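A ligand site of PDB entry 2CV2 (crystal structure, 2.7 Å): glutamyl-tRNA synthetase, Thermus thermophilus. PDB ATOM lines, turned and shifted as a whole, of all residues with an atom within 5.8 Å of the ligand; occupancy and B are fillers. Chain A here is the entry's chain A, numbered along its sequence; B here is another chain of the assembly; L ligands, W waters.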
ATOM      1  N   ARG A   5     -33.182 -11.151 -33.020  1.00  0.00           N
ATOM      2  CA  ARG A   5     -33.102 -11.702 -31.676  1.00  0.00           C
ATOM      3  C   ARG A   5     -32.979 -10.684 -30.576  1.00  0.00           C
ATOM      4  O   ARG A   5     -32.603  -9.546 -30.813  1.00  0.00           O
ATOM      5  CB  ARG A   5     -31.948 -12.688 -31.513  1.00  0.00           C
ATOM      6  CG  ARG A   5     -30.568 -12.215 -31.954  1.00  0.00           C
ATOM      7  CD  ARG A   5     -30.187 -10.826 -31.511  1.00  0.00           C
ATOM      8  NE  ARG A   5     -28.776 -10.543 -31.785  1.00  0.00           N
ATOM      9  CZ  ARG A   5     -28.176  -9.420 -31.421  1.00  0.00           C
ATOM     10  NH1 ARG A   5     -28.863  -8.477 -30.778  1.00  0.00           N
ATOM     11  NH2 ARG A   5     -26.893  -9.235 -31.650  1.00  0.00           N
ATOM     12  N   ILE A   6     -33.338 -11.128 -29.383  1.00  0.00           N
ATOM     13  CA  ILE A   6     -33.233 -10.320 -28.183  1.00  0.00           C
ATOM     14  C   ILE A   6     -32.225 -11.167 -27.376  1.00  0.00           C
ATOM     15  O   ILE A   6     -32.393 -12.393 -27.209  1.00  0.00           O
ATOM     16  CB  ILE A   6     -34.614 -10.167 -27.469  1.00  0.00           C
ATOM     17  CG1 ILE A   6     -34.519  -9.159 -26.324  1.00  0.00           C
ATOM     18  CG2 ILE A   6     -35.128 -11.499 -26.996  1.00  0.00           C
ATOM     19  CD1 ILE A   6     -34.174  -7.756 -26.760  1.00  0.00           C
ATOM     20  N   ALA A   7     -31.133 -10.529 -26.957  1.00  0.00           N
ATOM     21  CA  ALA A   7     -30.086 -11.222 -26.227  1.00  0.00           C
ATOM     22  C   ALA A   7     -29.924 -10.637 -24.839  1.00  0.00           C
ATOM     23  O   ALA A   7     -28.905 -10.047 -24.535  1.00  0.00           O
ATOM     24  CB  ALA A   7     -28.769 -11.102 -27.003  1.00  0.00           C
ATOM     25  N   PRO A   8     -30.931 -10.799 -23.969  1.00  0.00           N
ATOM     26  CA  PRO A   8     -30.907 -10.280 -22.602  1.00  0.00           C
ATOM     27  C   PRO A   8     -29.752 -10.839 -21.815  1.00  0.00           C
ATOM     28  O   PRO A   8     -29.292 -11.959 -22.063  1.00  0.00           O
ATOM     29  CB  PRO A   8     -32.217 -10.776 -21.990  1.00  0.00           C
ATOM     30  CG  PRO A   8     -33.046 -11.177 -23.136  1.00  0.00           C
ATOM     31  CD  PRO A   8     -32.102 -11.668 -24.181  1.00  0.00           C
ATOM     32  N   SER A   9     -29.303 -10.052 -20.841  1.00  0.00           N
ATOM     33  CA  SER A   9     -28.228 -10.464 -19.955  1.00  0.00           C
ATOM     34  C   SER A   9     -28.875 -10.630 -18.556  1.00  0.00           C
ATOM     35  O   SER A   9     -29.276  -9.652 -17.943  1.00  0.00           O
ATOM     36  CB  SER A   9     -27.170  -9.373 -19.967  1.00  0.00           C
ATOM     37  OG  SER A   9     -26.423  -9.350 -18.763  1.00  0.00           O
ATOM     38  N   PRO A  10     -28.971 -11.870 -18.047  1.00  0.00           N
ATOM     39  CA  PRO A  10     -29.576 -12.125 -16.726  1.00  0.00           C
ATOM     40  C   PRO A  10     -28.786 -11.547 -15.531  1.00  0.00           C
ATOM     41  O   PRO A  10     -28.077 -12.264 -14.828  1.00  0.00           O
ATOM     42  CB  PRO A  10     -29.656 -13.643 -16.687  1.00  0.00           C
ATOM     43  CG  PRO A  10     -28.362 -14.019 -17.336  1.00  0.00           C
ATOM     44  CD  PRO A  10     -28.278 -13.078 -18.528  1.00  0.00           C
ATOM     45  N   THR A  11     -28.955 -10.257 -15.299  1.00  0.00           N
ATOM     46  CA  THR A  11     -28.243  -9.587 -14.237  1.00  0.00           C
ATOM     47  C   THR A  11     -29.075  -8.710 -13.319  1.00  0.00           C
ATOM     48  O   THR A  11     -28.518  -7.906 -12.585  1.00  0.00           O
ATOM     49  CB  THR A  11     -27.109  -8.725 -14.841  1.00  0.00           C
ATOM     50  OG1 THR A  11     -27.698  -7.716 -15.693  1.00  0.00           O
ATOM     51  CG2 THR A  11     -26.129  -9.608 -15.647  1.00  0.00           C
ATOM     52  N   HIS A  15     -35.628  -5.769 -17.405  1.00  0.00           N
ATOM     53  CA  HIS A  15     -35.533  -4.362 -17.789  1.00  0.00           C
ATOM     54  C   HIS A  15     -36.493  -3.890 -18.881  1.00  0.00           C
ATOM     55  O   HIS A  15     -36.615  -4.529 -19.911  1.00  0.00           O
ATOM     56  CB  HIS A  15     -34.094  -4.083 -18.189  1.00  0.00           C
ATOM     57  CG  HIS A  15     -33.670  -2.675 -17.956  1.00  0.00           C
ATOM     58  ND1 HIS A  15     -33.947  -1.659 -18.846  1.00  0.00           N
ATOM     59  CD2 HIS A  15     -33.041  -2.096 -16.901  1.00  0.00           C
ATOM     60  CE1 HIS A  15     -33.499  -0.513 -18.348  1.00  0.00           C
ATOM     61  NE2 HIS A  15     -32.949  -0.754 -17.179  1.00  0.00           N
ATOM     62  N   GLY A  17     -36.084  -1.701 -20.926  1.00  0.00           N
ATOM     63  CA  GLY A  17     -35.338  -1.462 -22.151  1.00  0.00           C
ATOM     64  C   GLY A  17     -35.299  -2.742 -22.963  1.00  0.00           C
ATOM     65  O   GLY A  17     -35.226  -2.710 -24.197  1.00  0.00           O
ATOM     66  N   THR A  18     -35.329  -3.864 -22.241  1.00  0.00           N
ATOM     67  CA  THR A  18     -35.317  -5.179 -22.853  1.00  0.00           C
ATOM     68  C   THR A  18     -36.620  -5.411 -23.549  1.00  0.00           C
ATOM     69  O   THR A  18     -36.631  -5.962 -24.637  1.00  0.00           O
ATOM     70  CB  THR A  18     -35.147  -6.274 -21.812  1.00  0.00           C
ATOM     71  OG1 THR A  18     -33.834  -6.187 -21.285  1.00  0.00           O
ATOM     72  CG2 THR A  18     -35.267  -7.629 -22.439  1.00  0.00           C
ATOM     73  N   TYR A  20     -38.683  -3.080 -24.672  1.00  0.00           N
ATOM     74  CA  TYR A  20     -38.677  -2.129 -25.758  1.00  0.00           C
ATOM     75  C   TYR A  20     -37.932  -2.632 -26.981  1.00  0.00           C
ATOM     76  O   TYR A  20     -38.451  -2.571 -28.104  1.00  0.00           O
ATOM     77  CB  TYR A  20     -38.052  -0.843 -25.279  1.00  0.00           C
ATOM     78  CG  TYR A  20     -37.736   0.155 -26.338  1.00  0.00           C
ATOM     79  CD1 TYR A  20     -38.751   0.843 -26.980  1.00  0.00           C
ATOM     80  CD2 TYR A  20     -36.420   0.468 -26.650  1.00  0.00           C
ATOM     81  CE1 TYR A  20     -38.477   1.841 -27.918  1.00  0.00           C
ATOM     82  CE2 TYR A  20     -36.123   1.467 -27.587  1.00  0.00           C
ATOM     83  CZ  TYR A  20     -37.169   2.138 -28.216  1.00  0.00           C
ATOM     84  OH  TYR A  20     -36.909   3.134 -29.134  1.00  0.00           O
ATOM     85  N   ILE A  21     -36.720  -3.133 -26.789  1.00  0.00           N
ATOM     86  CA  ILE A  21     -35.962  -3.612 -27.931  1.00  0.00           C
ATOM     87  C   ILE A  21     -36.598  -4.892 -28.498  1.00  0.00           C
ATOM     88  O   ILE A  21     -36.732  -5.037 -29.715  1.00  0.00           O
ATOM     89  CB  ILE A  21     -34.470  -3.861 -27.560  1.00  0.00           C
ATOM     90  CG1 ILE A  21     -33.757  -2.516 -27.362  1.00  0.00           C
ATOM     91  CG2 ILE A  21     -33.765  -4.647 -28.626  1.00  0.00           C
ATOM     92  CD1 ILE A  21     -33.724  -1.651 -28.598  1.00  0.00           C
ATOM     93  N   ARG A  39     -31.849 -15.319 -27.000  1.00  0.00           N
ATOM     94  CA  ARG A  39     -30.551 -15.883 -26.608  1.00  0.00           C
ATOM     95  C   ARG A  39     -30.179 -15.262 -25.280  1.00  0.00           C
ATOM     96  O   ARG A  39     -30.117 -14.036 -25.180  1.00  0.00           O
ATOM     97  CB  ARG A  39     -29.440 -15.553 -27.619  1.00  0.00           C
ATOM     98  CG  ARG A  39     -28.069 -16.093 -27.214  1.00  0.00           C
ATOM     99  CD  ARG A  39     -26.943 -16.015 -28.279  1.00  0.00           C
ATOM    100  NE  ARG A  39     -26.523 -14.660 -28.607  1.00  0.00           N
ATOM    101  CZ  ARG A  39     -26.737 -14.084 -29.775  1.00  0.00           C
ATOM    102  NH1 ARG A  39     -27.359 -14.750 -30.741  1.00  0.00           N
ATOM    103  NH2 ARG A  39     -26.358 -12.831 -29.995  1.00  0.00           N
ATOM    104  N   GLU A  41     -27.676 -14.182 -22.583  1.00  0.00           N
ATOM    105  CA  GLU A  41     -26.262 -13.891 -22.509  1.00  0.00           C
ATOM    106  C   GLU A  41     -25.766 -13.835 -21.067  1.00  0.00           C
ATOM    107  O   GLU A  41     -25.645 -12.768 -20.454  1.00  0.00           O
ATOM    108  CB  GLU A  41     -25.984 -12.596 -23.278  1.00  0.00           C
ATOM    109  CG  GLU A  41     -26.522 -12.634 -24.725  1.00  0.00           C
ATOM    110  CD  GLU A  41     -25.646 -11.902 -25.759  1.00  0.00           C
ATOM    111  OE1 GLU A  41     -25.136 -10.805 -25.450  1.00  0.00           O
ATOM    112  OE2 GLU A  41     -25.500 -12.410 -26.909  1.00  0.00           O
ATOM    113  N   TYR A 187     -18.667 -10.327 -24.189  1.00  0.00           N
ATOM    114  CA  TYR A 187     -19.803 -10.023 -25.017  1.00  0.00           C
ATOM    115  C   TYR A 187     -19.402 -10.031 -26.509  1.00  0.00           C
ATOM    116  O   TYR A 187     -20.027 -10.685 -27.317  1.00  0.00           O
ATOM    117  CB  TYR A 187     -20.349  -8.640 -24.650  1.00  0.00           C
ATOM    118  CG  TYR A 187     -21.283  -8.066 -25.690  1.00  0.00           C
ATOM    119  CD1 TYR A 187     -22.633  -8.447 -25.727  1.00  0.00           C
ATOM    120  CD2 TYR A 187     -20.809  -7.180 -26.680  1.00  0.00           C
ATOM    121  CE1 TYR A 187     -23.472  -7.969 -26.702  1.00  0.00           C
ATOM    122  CE2 TYR A 187     -21.652  -6.698 -27.669  1.00  0.00           C
ATOM    123  CZ  TYR A 187     -22.984  -7.097 -27.677  1.00  0.00           C
ATOM    124  OH  TYR A 187     -23.832  -6.617 -28.650  1.00  0.00           O
ATOM    125  N   ASN A 191     -21.210 -12.655 -29.074  1.00  0.00           N
ATOM    126  CA  ASN A 191     -22.211 -12.033 -29.910  1.00  0.00           C
ATOM    127  C   ASN A 191     -22.078 -12.329 -31.388  1.00  0.00           C
ATOM    128  O   ASN A 191     -23.059 -12.670 -32.043  1.00  0.00           O
ATOM    129  CB  ASN A 191     -22.187 -10.534 -29.657  1.00  0.00           C
ATOM    130  CG  ASN A 191     -23.528  -9.886 -29.941  1.00  0.00           C
ATOM    131  OD1 ASN A 191     -23.779  -9.436 -31.065  1.00  0.00           O
ATOM    132  ND2 ASN A 191     -24.411  -9.835 -28.919  1.00  0.00           N
ATOM    133  N   ASP A 195     -24.425 -14.870 -33.266  1.00  0.00           N
ATOM    134  CA  ASP A 195     -25.322 -14.297 -34.235  1.00  0.00           C
ATOM    135  C   ASP A 195     -25.133 -15.018 -35.553  1.00  0.00           C
ATOM    136  O   ASP A 195     -26.086 -15.292 -36.275  1.00  0.00           O
ATOM    137  CB  ASP A 195     -25.054 -12.810 -34.421  1.00  0.00           C
ATOM    138  CG  ASP A 195     -25.821 -11.945 -33.412  1.00  0.00           C
ATOM    139  OD1 ASP A 195     -25.485 -10.739 -33.354  1.00  0.00           O
ATOM    140  OD2 ASP A 195     -26.748 -12.442 -32.702  1.00  0.00           O
ATOM    141  N   VAL A 203     -29.665  -7.268 -36.841  1.00  0.00           N
ATOM    142  CA  VAL A 203     -29.368  -6.959 -35.461  1.00  0.00           C
ATOM    143  C   VAL A 203     -29.945  -5.591 -35.057  1.00  0.00           C
ATOM    144  O   VAL A 203     -29.548  -4.556 -35.569  1.00  0.00           O
ATOM    145  CB  VAL A 203     -27.858  -6.976 -35.229  1.00  0.00           C
ATOM    146  CG1 VAL A 203     -27.551  -6.474 -33.821  1.00  0.00           C
ATOM    147  CG2 VAL A 203     -27.321  -8.382 -35.438  1.00  0.00           C
ATOM    148  N   ILE A 204     -30.902  -5.627 -34.136  1.00  0.00           N
ATOM    149  CA  ILE A 204     -31.577  -4.428 -33.632  1.00  0.00           C
ATOM    150  C   ILE A 204     -31.283  -4.409 -32.134  1.00  0.00           C
ATOM    151  O   ILE A 204     -31.664  -5.315 -31.405  1.00  0.00           O
ATOM    152  CB  ILE A 204     -33.089  -4.551 -33.865  1.00  0.00           C
ATOM    153  CG1 ILE A 204     -33.360  -4.917 -35.324  1.00  0.00           C
ATOM    154  CG2 ILE A 204     -33.788  -3.275 -33.486  1.00  0.00           C
ATOM    155  CD1 ILE A 204     -34.752  -5.490 -35.563  1.00  0.00           C
ATOM    156  N   ARG A 205     -30.581  -3.380 -31.684  1.00  0.00           N
ATOM    157  CA  ARG A 205     -30.215  -3.257 -30.272  1.00  0.00           C
ATOM    158  C   ARG A 205     -30.147  -1.745 -30.023  1.00  0.00           C
ATOM    159  O   ARG A 205     -30.180  -0.980 -30.989  1.00  0.00           O
ATOM    160  CB  ARG A 205     -28.869  -3.939 -30.046  1.00  0.00           C
ATOM    161  CG  ARG A 205     -27.704  -3.071 -30.426  1.00  0.00           C
ATOM    162  CD  ARG A 205     -26.849  -3.591 -31.551  1.00  0.00           C
ATOM    163  NE  ARG A 205     -25.965  -4.682 -31.143  1.00  0.00           N
ATOM    164  CZ  ARG A 205     -24.753  -4.905 -31.644  1.00  0.00           C
ATOM    165  NH1 ARG A 205     -24.229  -4.144 -32.593  1.00  0.00           N
ATOM    166  NH2 ARG A 205     -24.058  -5.948 -31.214  1.00  0.00           N
ATOM    167  N   ALA A 206     -30.053  -1.290 -28.789  1.00  0.00           N
ATOM    168  CA  ALA A 206     -30.014   0.158 -28.588  1.00  0.00           C
ATOM    169  C   ALA A 206     -28.701   0.762 -28.977  1.00  0.00           C
ATOM    170  O   ALA A 206     -27.676   0.090 -29.036  1.00  0.00           O
ATOM    171  CB  ALA A 206     -30.344   0.532 -27.153  1.00  0.00           C
ATOM    172  N   GLU A 207     -28.763   2.056 -29.241  1.00  0.00           N
ATOM    173  CA  GLU A 207     -27.647   2.915 -29.632  1.00  0.00           C
ATOM    174  C   GLU A 207     -26.386   2.854 -28.721  1.00  0.00           C
ATOM    175  O   GLU A 207     -25.281   3.215 -29.127  1.00  0.00           O
ATOM    176  CB  GLU A 207     -28.183   4.339 -29.688  1.00  0.00           C
ATOM    177  CG  GLU A 207     -27.225   5.354 -30.251  1.00  0.00           C
ATOM    178  CD  GLU A 207     -27.737   6.788 -30.134  1.00  0.00           C
ATOM    179  OE1 GLU A 207     -27.086   7.705 -30.695  1.00  0.00           O
ATOM    180  OE2 GLU A 207     -28.785   7.007 -29.480  1.00  0.00           O
ATOM    181  N   GLU A 208     -26.539   2.397 -27.490  1.00  0.00           N
ATOM    182  CA  GLU A 208     -25.383   2.309 -26.615  1.00  0.00           C
ATOM    183  C   GLU A 208     -24.293   1.407 -27.208  1.00  0.00           C
ATOM    184  O   GLU A 208     -23.146   1.445 -26.787  1.00  0.00           O
ATOM    185  CB  GLU A 208     -25.816   1.759 -25.257  1.00  0.00           C
ATOM    186  CG  GLU A 208     -26.166   0.286 -25.295  1.00  0.00           C
ATOM    187  CD  GLU A 208     -26.880  -0.178 -24.059  1.00  0.00           C
ATOM    188  OE1 GLU A 208     -26.691   0.444 -22.987  1.00  0.00           O
ATOM    189  OE2 GLU A 208     -27.623  -1.178 -24.140  1.00  0.00           O
ATOM    190  N   TRP A 209     -24.672   0.587 -28.183  1.00  0.00           N
ATOM    191  CA  TRP A 209     -23.758  -0.335 -28.832  1.00  0.00           C
ATOM    192  C   TRP A 209     -23.116   0.108 -30.135  1.00  0.00           C
ATOM    193  O   TRP A 209     -22.201  -0.589 -30.620  1.00  0.00           O
ATOM    194  CB  TRP A 209     -24.465  -1.652 -29.140  1.00  0.00           C
ATOM    195  CG  TRP A 209     -24.871  -2.389 -27.945  1.00  0.00           C
ATOM    196  CD1 TRP A 209     -26.127  -2.496 -27.447  1.00  0.00           C
ATOM    197  CD2 TRP A 209     -24.017  -3.105 -27.058  1.00  0.00           C
ATOM    198  NE1 TRP A 209     -26.118  -3.234 -26.297  1.00  0.00           N
ATOM    199  CE2 TRP A 209     -24.839  -3.618 -26.032  1.00  0.00           C
ATOM    200  CE3 TRP A 209     -22.644  -3.358 -27.033  1.00  0.00           C
ATOM    201  CZ2 TRP A 209     -24.320  -4.384 -24.980  1.00  0.00           C
ATOM    202  CZ3 TRP A 209     -22.125  -4.124 -25.981  1.00  0.00           C
ATOM    203  CH2 TRP A 209     -22.980  -4.629 -24.958  1.00  0.00           C
ATOM    204  N   PRO A 234     -32.960   4.128 -30.154  1.00  0.00           N
ATOM    205  CA  PRO A 234     -32.583   5.110 -29.140  1.00  0.00           C
ATOM    206  C   PRO A 234     -32.743   4.545 -27.737  1.00  0.00           C
ATOM    207  O   PRO A 234     -33.556   3.643 -27.528  1.00  0.00           O
ATOM    208  CB  PRO A 234     -33.536   6.270 -29.443  1.00  0.00           C
ATOM    209  CG  PRO A 234     -34.786   5.561 -29.907  1.00  0.00           C
ATOM    210  CD  PRO A 234     -34.230   4.488 -30.814  1.00  0.00           C
ATOM    211  N   LEU A 235     -31.960   5.058 -26.791  1.00  0.00           N
ATOM    212  CA  LEU A 235     -32.027   4.621 -25.398  1.00  0.00           C
ATOM    213  C   LEU A 235     -33.171   5.288 -24.646  1.00  0.00           C
ATOM    214  O   LEU A 235     -33.329   6.517 -24.735  1.00  0.00           O
ATOM    215  CB  LEU A 235     -30.777   5.022 -24.629  1.00  0.00           C
ATOM    216  CG  LEU A 235     -29.459   4.279 -24.681  1.00  0.00           C
ATOM    217  CD1 LEU A 235     -29.714   2.783 -24.686  1.00  0.00           C
ATOM    218  CD2 LEU A 235     -28.704   4.719 -25.882  1.00  0.00           C
ATOM    219  N   LEU A 236     -33.927   4.507 -23.904  1.00  0.00           N
ATOM    220  CA  LEU A 236     -34.992   5.061 -23.094  1.00  0.00           C
ATOM    221  C   LEU A 236     -34.291   5.886 -21.985  1.00  0.00           C
ATOM    222  O   LEU A 236     -33.196   5.514 -21.526  1.00  0.00           O
ATOM    223  CB  LEU A 236     -35.799   3.941 -22.487  1.00  0.00           C
ATOM    224  CG  LEU A 236     -37.078   3.477 -23.164  1.00  0.00           C
ATOM    225  CD1 LEU A 236     -37.019   3.624 -24.654  1.00  0.00           C
ATOM    226  CD2 LEU A 236     -37.316   2.045 -22.748  1.00  0.00           C
ATOM    227  N   ARG A 237     -34.906   7.001 -21.571  1.00  0.00           N
ATOM    228  CA  ARG A 237     -34.310   7.896 -20.569  1.00  0.00           C
ATOM    229  C   ARG A 237     -35.125   8.141 -19.306  1.00  0.00           C
ATOM    230  O   ARG A 237     -36.349   7.941 -19.285  1.00  0.00           O
ATOM    231  CB  ARG A 237     -34.050   9.285 -21.197  1.00  0.00           C
ATOM    232  CG  ARG A 237     -33.344   9.302 -22.520  1.00  0.00           C
ATOM    233  CD  ARG A 237     -32.004   8.610 -22.449  1.00  0.00           C
ATOM    234  NE  ARG A 237     -31.354   8.694 -23.749  1.00  0.00           N
ATOM    235  CZ  ARG A 237     -30.762   9.780 -24.195  1.00  0.00           C
ATOM    236  NH1 ARG A 237     -30.715  10.858 -23.439  1.00  0.00           N
ATOM    237  NH2 ARG A 237     -30.268   9.806 -25.422  1.00  0.00           N
ATOM    238  N   LYS A 243     -29.740   8.007 -19.346  1.00  0.00           N
ATOM    239  CA  LYS A 243     -30.157   6.645 -19.700  1.00  0.00           C
ATOM    240  C   LYS A 243     -30.990   6.135 -18.531  1.00  0.00           C
ATOM    241  O   LYS A 243     -30.559   6.200 -17.381  1.00  0.00           O
ATOM    242  CB  LYS A 243     -28.955   5.749 -19.881  1.00  0.00           C
ATOM    243  CG  LYS A 243     -29.189   4.527 -20.725  1.00  0.00           C
ATOM    244  CD  LYS A 243     -27.950   3.651 -20.759  1.00  0.00           C
ATOM    245  CE  LYS A 243     -27.609   3.165 -19.351  1.00  0.00           C
ATOM    246  NZ  LYS A 243     -26.679   2.008 -19.395  1.00  0.00           N
ATOM    247  N   ILE A 244     -32.175   5.635 -18.826  1.00  0.00           N
ATOM    248  CA  ILE A 244     -33.079   5.166 -17.776  1.00  0.00           C
ATOM    249  C   ILE A 244     -32.358   4.226 -16.801  1.00  0.00           C
ATOM    250  O   ILE A 244     -31.527   3.429 -17.210  1.00  0.00           O
ATOM    251  CB  ILE A 244     -34.330   4.522 -18.445  1.00  0.00           C
ATOM    252  CG1 ILE A 244     -35.538   4.640 -17.513  1.00  0.00           C
ATOM    253  CG2 ILE A 244     -34.041   3.070 -18.863  1.00  0.00           C
ATOM    254  CD1 ILE A 244     -36.845   4.222 -18.168  1.00  0.00           C
ATOM    255  P     A B  75     -19.501  -9.619 -20.350  1.00  0.00           P
ATOM    256  OP1   A B  75     -18.977 -11.003 -20.401  1.00  0.00           O
ATOM    257  OP2   A B  75     -19.218  -8.683 -21.470  1.00  0.00           O
ATOM    258  O5'   A B  75     -21.078  -9.688 -20.090  1.00  0.00           O
ATOM    259  C5'   A B  75     -21.996  -9.567 -21.150  1.00  0.00           C
ATOM    260  C4'   A B  75     -23.019  -8.514 -20.821  1.00  0.00           C
ATOM    261  O4'   A B  75     -22.374  -7.360 -20.231  1.00  0.00           O
ATOM    262  C3'   A B  75     -23.703  -7.987 -22.065  1.00  0.00           C
ATOM    263  O3'   A B  75     -24.668  -8.965 -22.461  1.00  0.00           O
ATOM    264  C2'   A B  75     -24.082  -6.568 -21.673  1.00  0.00           C
ATOM    265  O2'   A B  75     -25.305  -6.439 -20.957  1.00  0.00           O
ATOM    266  C1'   A B  75     -22.905  -6.169 -20.780  1.00  0.00           C
ATOM    267  N9    A B  75     -21.834  -5.499 -21.526  1.00  0.00           N
ATOM    268  C8    A B  75     -20.619  -6.034 -21.886  1.00  0.00           C
ATOM    269  N7    A B  75     -19.876  -5.220 -22.590  1.00  0.00           N
ATOM    270  C5    A B  75     -20.644  -4.067 -22.686  1.00  0.00           C
ATOM    271  C6    A B  75     -20.429  -2.824 -23.342  1.00  0.00           C
ATOM    272  N6    A B  75     -19.328  -2.534 -24.045  1.00  0.00           N
ATOM    273  N1    A B  75     -21.397  -1.885 -23.248  1.00  0.00           N
ATOM    274  C2    A B  75     -22.506  -2.184 -22.561  1.00  0.00           C
ATOM    275  N3    A B  75     -22.834  -3.309 -21.912  1.00  0.00           N
ATOM    276  C4    A B  75     -21.845  -4.221 -22.020  1.00  0.00           C
HETATM  277  C1  LIG L   1     -33.301   0.986 -24.749  1.00  0.00           C
HETATM  278  S1  LIG L   1     -29.080  -6.249 -21.830  1.00  0.00           S
HETATM  279  N1  LIG L   1     -26.602  -9.029 -23.989  1.00  0.00           N
HETATM  280  C2  LIG L   1     -26.426  -7.655 -24.516  1.00  0.00           C
HETATM  281  C3  LIG L   1     -27.011  -7.775 -25.940  1.00  0.00           C
HETATM  282  C4  LIG L   1     -26.617  -6.724 -26.956  1.00  0.00           C
HETATM  283  C5  LIG L   1     -27.117  -7.073 -28.342  1.00  0.00           C
HETATM  284  O1  LIG L   1     -26.364  -7.218 -29.294  1.00  0.00           O
HETATM  285  O2  LIG L   1     -28.412  -7.214 -28.451  1.00  0.00           O
HETATM  286  C6  LIG L   1     -27.278  -6.616 -23.753  1.00  0.00           C
HETATM  287  O3  LIG L   1     -27.281  -5.399 -23.998  1.00  0.00           O
HETATM  288  N2  LIG L   1     -28.061  -7.140 -22.790  1.00  0.00           N
HETATM  289  O4  LIG L   1     -28.299  -5.277 -21.090  1.00  0.00           O
HETATM  290  O5  LIG L   1     -29.796  -7.155 -20.929  1.00  0.00           O
HETATM  291  O6  LIG L   1     -30.113  -5.439 -22.717  1.00  0.00           O
HETATM  292  C7  LIG L   1     -30.756  -6.135 -23.730  1.00  0.00           C
HETATM  293  C8  LIG L   1     -31.345  -5.308 -24.851  1.00  0.00           C
HETATM  294  O7  LIG L   1     -31.995  -4.149 -24.320  1.00  0.00           O
HETATM  295  C9  LIG L   1     -31.298  -2.983 -24.778  1.00  0.00           C
HETATM  296  N3  LIG L   1     -31.338  -1.849 -23.761  1.00  0.00           N
HETATM  297  C10 LIG L   1     -32.013  -0.651 -23.890  1.00  0.00           C
HETATM  298  N4  LIG L   1     -32.775  -0.249 -24.944  1.00  0.00           N
HETATM  299  N5  LIG L   1     -33.140   1.787 -23.685  1.00  0.00           N
HETATM  300  C11 LIG L   1     -32.365   1.347 -22.638  1.00  0.00           C
HETATM  301  N6  LIG L   1     -32.191   2.151 -21.570  1.00  0.00           N
HETATM  302  C12 LIG L   1     -31.758   0.057 -22.737  1.00  0.00           C
HETATM  303  N7  LIG L   1     -30.965  -0.648 -21.904  1.00  0.00           N
HETATM  304  C13 LIG L   1     -30.731  -1.763 -22.555  1.00  0.00           C
HETATM  305  C14 LIG L   1     -29.866  -3.447 -25.196  1.00  0.00           C
HETATM  306  O8  LIG L   1     -29.235  -2.544 -26.093  1.00  0.00           O
HETATM  307  C15 LIG L   1     -30.207  -4.824 -25.741  1.00  0.00           C
HETATM  308  O9  LIG L   1     -30.634  -4.730 -27.094  1.00  0.00           O
HETATM  309  O   HOH W   1     -27.530  -2.989 -19.854  1.00  0.00           O
HETATM  310  O   HOH W   2     -30.809  -7.711 -27.397  1.00  0.00           O
HETATM  311  O   HOH W   3     -27.055  -6.265 -18.812  1.00  0.00           O
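O3' of A 75 of chain B is in hydrogen-bond range of a nitrogen (N1) of the ligand, 2.5 Å away.
O of Ala 7 lies within hydrogen-bond range of N1 of the ligand, 2.6 Å away.
The side-chain hydroxyl of Tyr 187 sits at hydrogen-bond distance from an oxygen (O1) of the ligand, at 2.7 Å.
An oxygen (O2) of the ligand is in salt-bridge range of the guanidinium group (NH1) of Arg 5 (2.7 Å).
The side-chain carboxylate (OE1) of Glu 41 is in salt-bridge range of a nitrogen (N1) of the ligand, 2.7 Å away.
A nitrogen (N5) of the ligand lies within hydrogen-bond range of the backbone NH (N) of Leu 236, 2.8 Å away.
OE2 of Glu 208 sits at hydrogen-bond distance from O8 of the ligand.
An oxygen (O5) of the ligand is in hydrogen-bond range of the backbone NH of Ser 9 (2.9 Å).
An oxygen (O8) of the ligand sits at hydrogen-bond distance from the backbone NH (N) of Ala 206.
The guanidinium group (NE) of Arg 205 lies within salt-bridge range of an oxygen (O1) of the ligand (3.2 Å).
O8 of the ligand sits at hydrogen-bond distance from NE1 of Trp 209, 3.2 Å away.
The side-chain amide nitrogen (ND2) of Asn 191 is in hydrogen-bond range of an oxygen (O1) of the ligand (3.3 Å).
The backbone NH (N) of Tyr 187 is in hydrogen-bond range of OP2 of A 75 of chain B (3.2 Å).
The side-chain amide nitrogen (ND2) of Asn 191 sits close to the side-chain hydroxyl (OH) of Tyr 187.
The side-chain carboxylate (OE2) of Glu 41 sits at hydrogen-bond distance from the side-chain amide nitrogen (ND2) of Asn 191.
The backbone carbonyl oxygen (O) of Pro 8 is in hydrogen-bond range of the backbone NH (N) of Glu 41, 2.8 Å away.
The guanidinium group (NE) of Arg 39 is in salt-bridge range of the side-chain carboxylate (OE2) of Glu 41.
N of Ile 244 is in hydrogen-bond range of O of Leu 236 (2.9 Å).
OE1 of Glu 208 lies within salt-bridge range of NZ of Lys 243 (3.9 Å).
N of Gly 17 sits at hydrogen-bond distance from ND1 of His 15, 3.0 Å away.
Pro 8 touches the ligand (CA to O5, 3.7 Å).
Gly 17 touches the ligand.
CA of Thr 18 touches O7 of the ligand, 3.8 Å away.
CD2 of Tyr 20 touches C1 of the ligand, at 3.7 Å.
Ile 21 touches the ligand (CG1 to N4, 3.5 Å).
Pro 234 touches the ligand.
CA of Leu 235 touches N5 of the ligand, 3.5 Å away.
CG of Lys 243 touches N6 of the ligand, 3.9 Å away.
Ile 244 touches the ligand.
Hydrophobic or aromatic side chains within 4 Å of the ligand: Ala 7, Tyr 20, Ile 21, Tyr 187, Ala 206, Trp 209, Leu 235, Leu 236 and Ile 244.
21 residues have an atom within 4 Å of the ligand: Arg 5, Ala 7, Pro 8, Ser 9, Gly 17, Thr 18, Tyr 20, Ile 21, Glu 41, Tyr 187, Asn 191, Arg 205, Ala 206, Glu 208, Trp 209, Pro 234, Leu 235, Leu 236, Lys 243, Ile 244 and A 75 of chain B.
The nearest printed residue that does not touch the ligand is Ile 6 (4.2 Å).
Water W2 bridges O2 of the ligand and N of Ala 7.
Water W3 lies within hydrogen-bond range of O2' of A 75 of chain B (2.8 Å), O4 of the ligand (2.8 Å) and OG of Ser 9 (3.1 Å).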
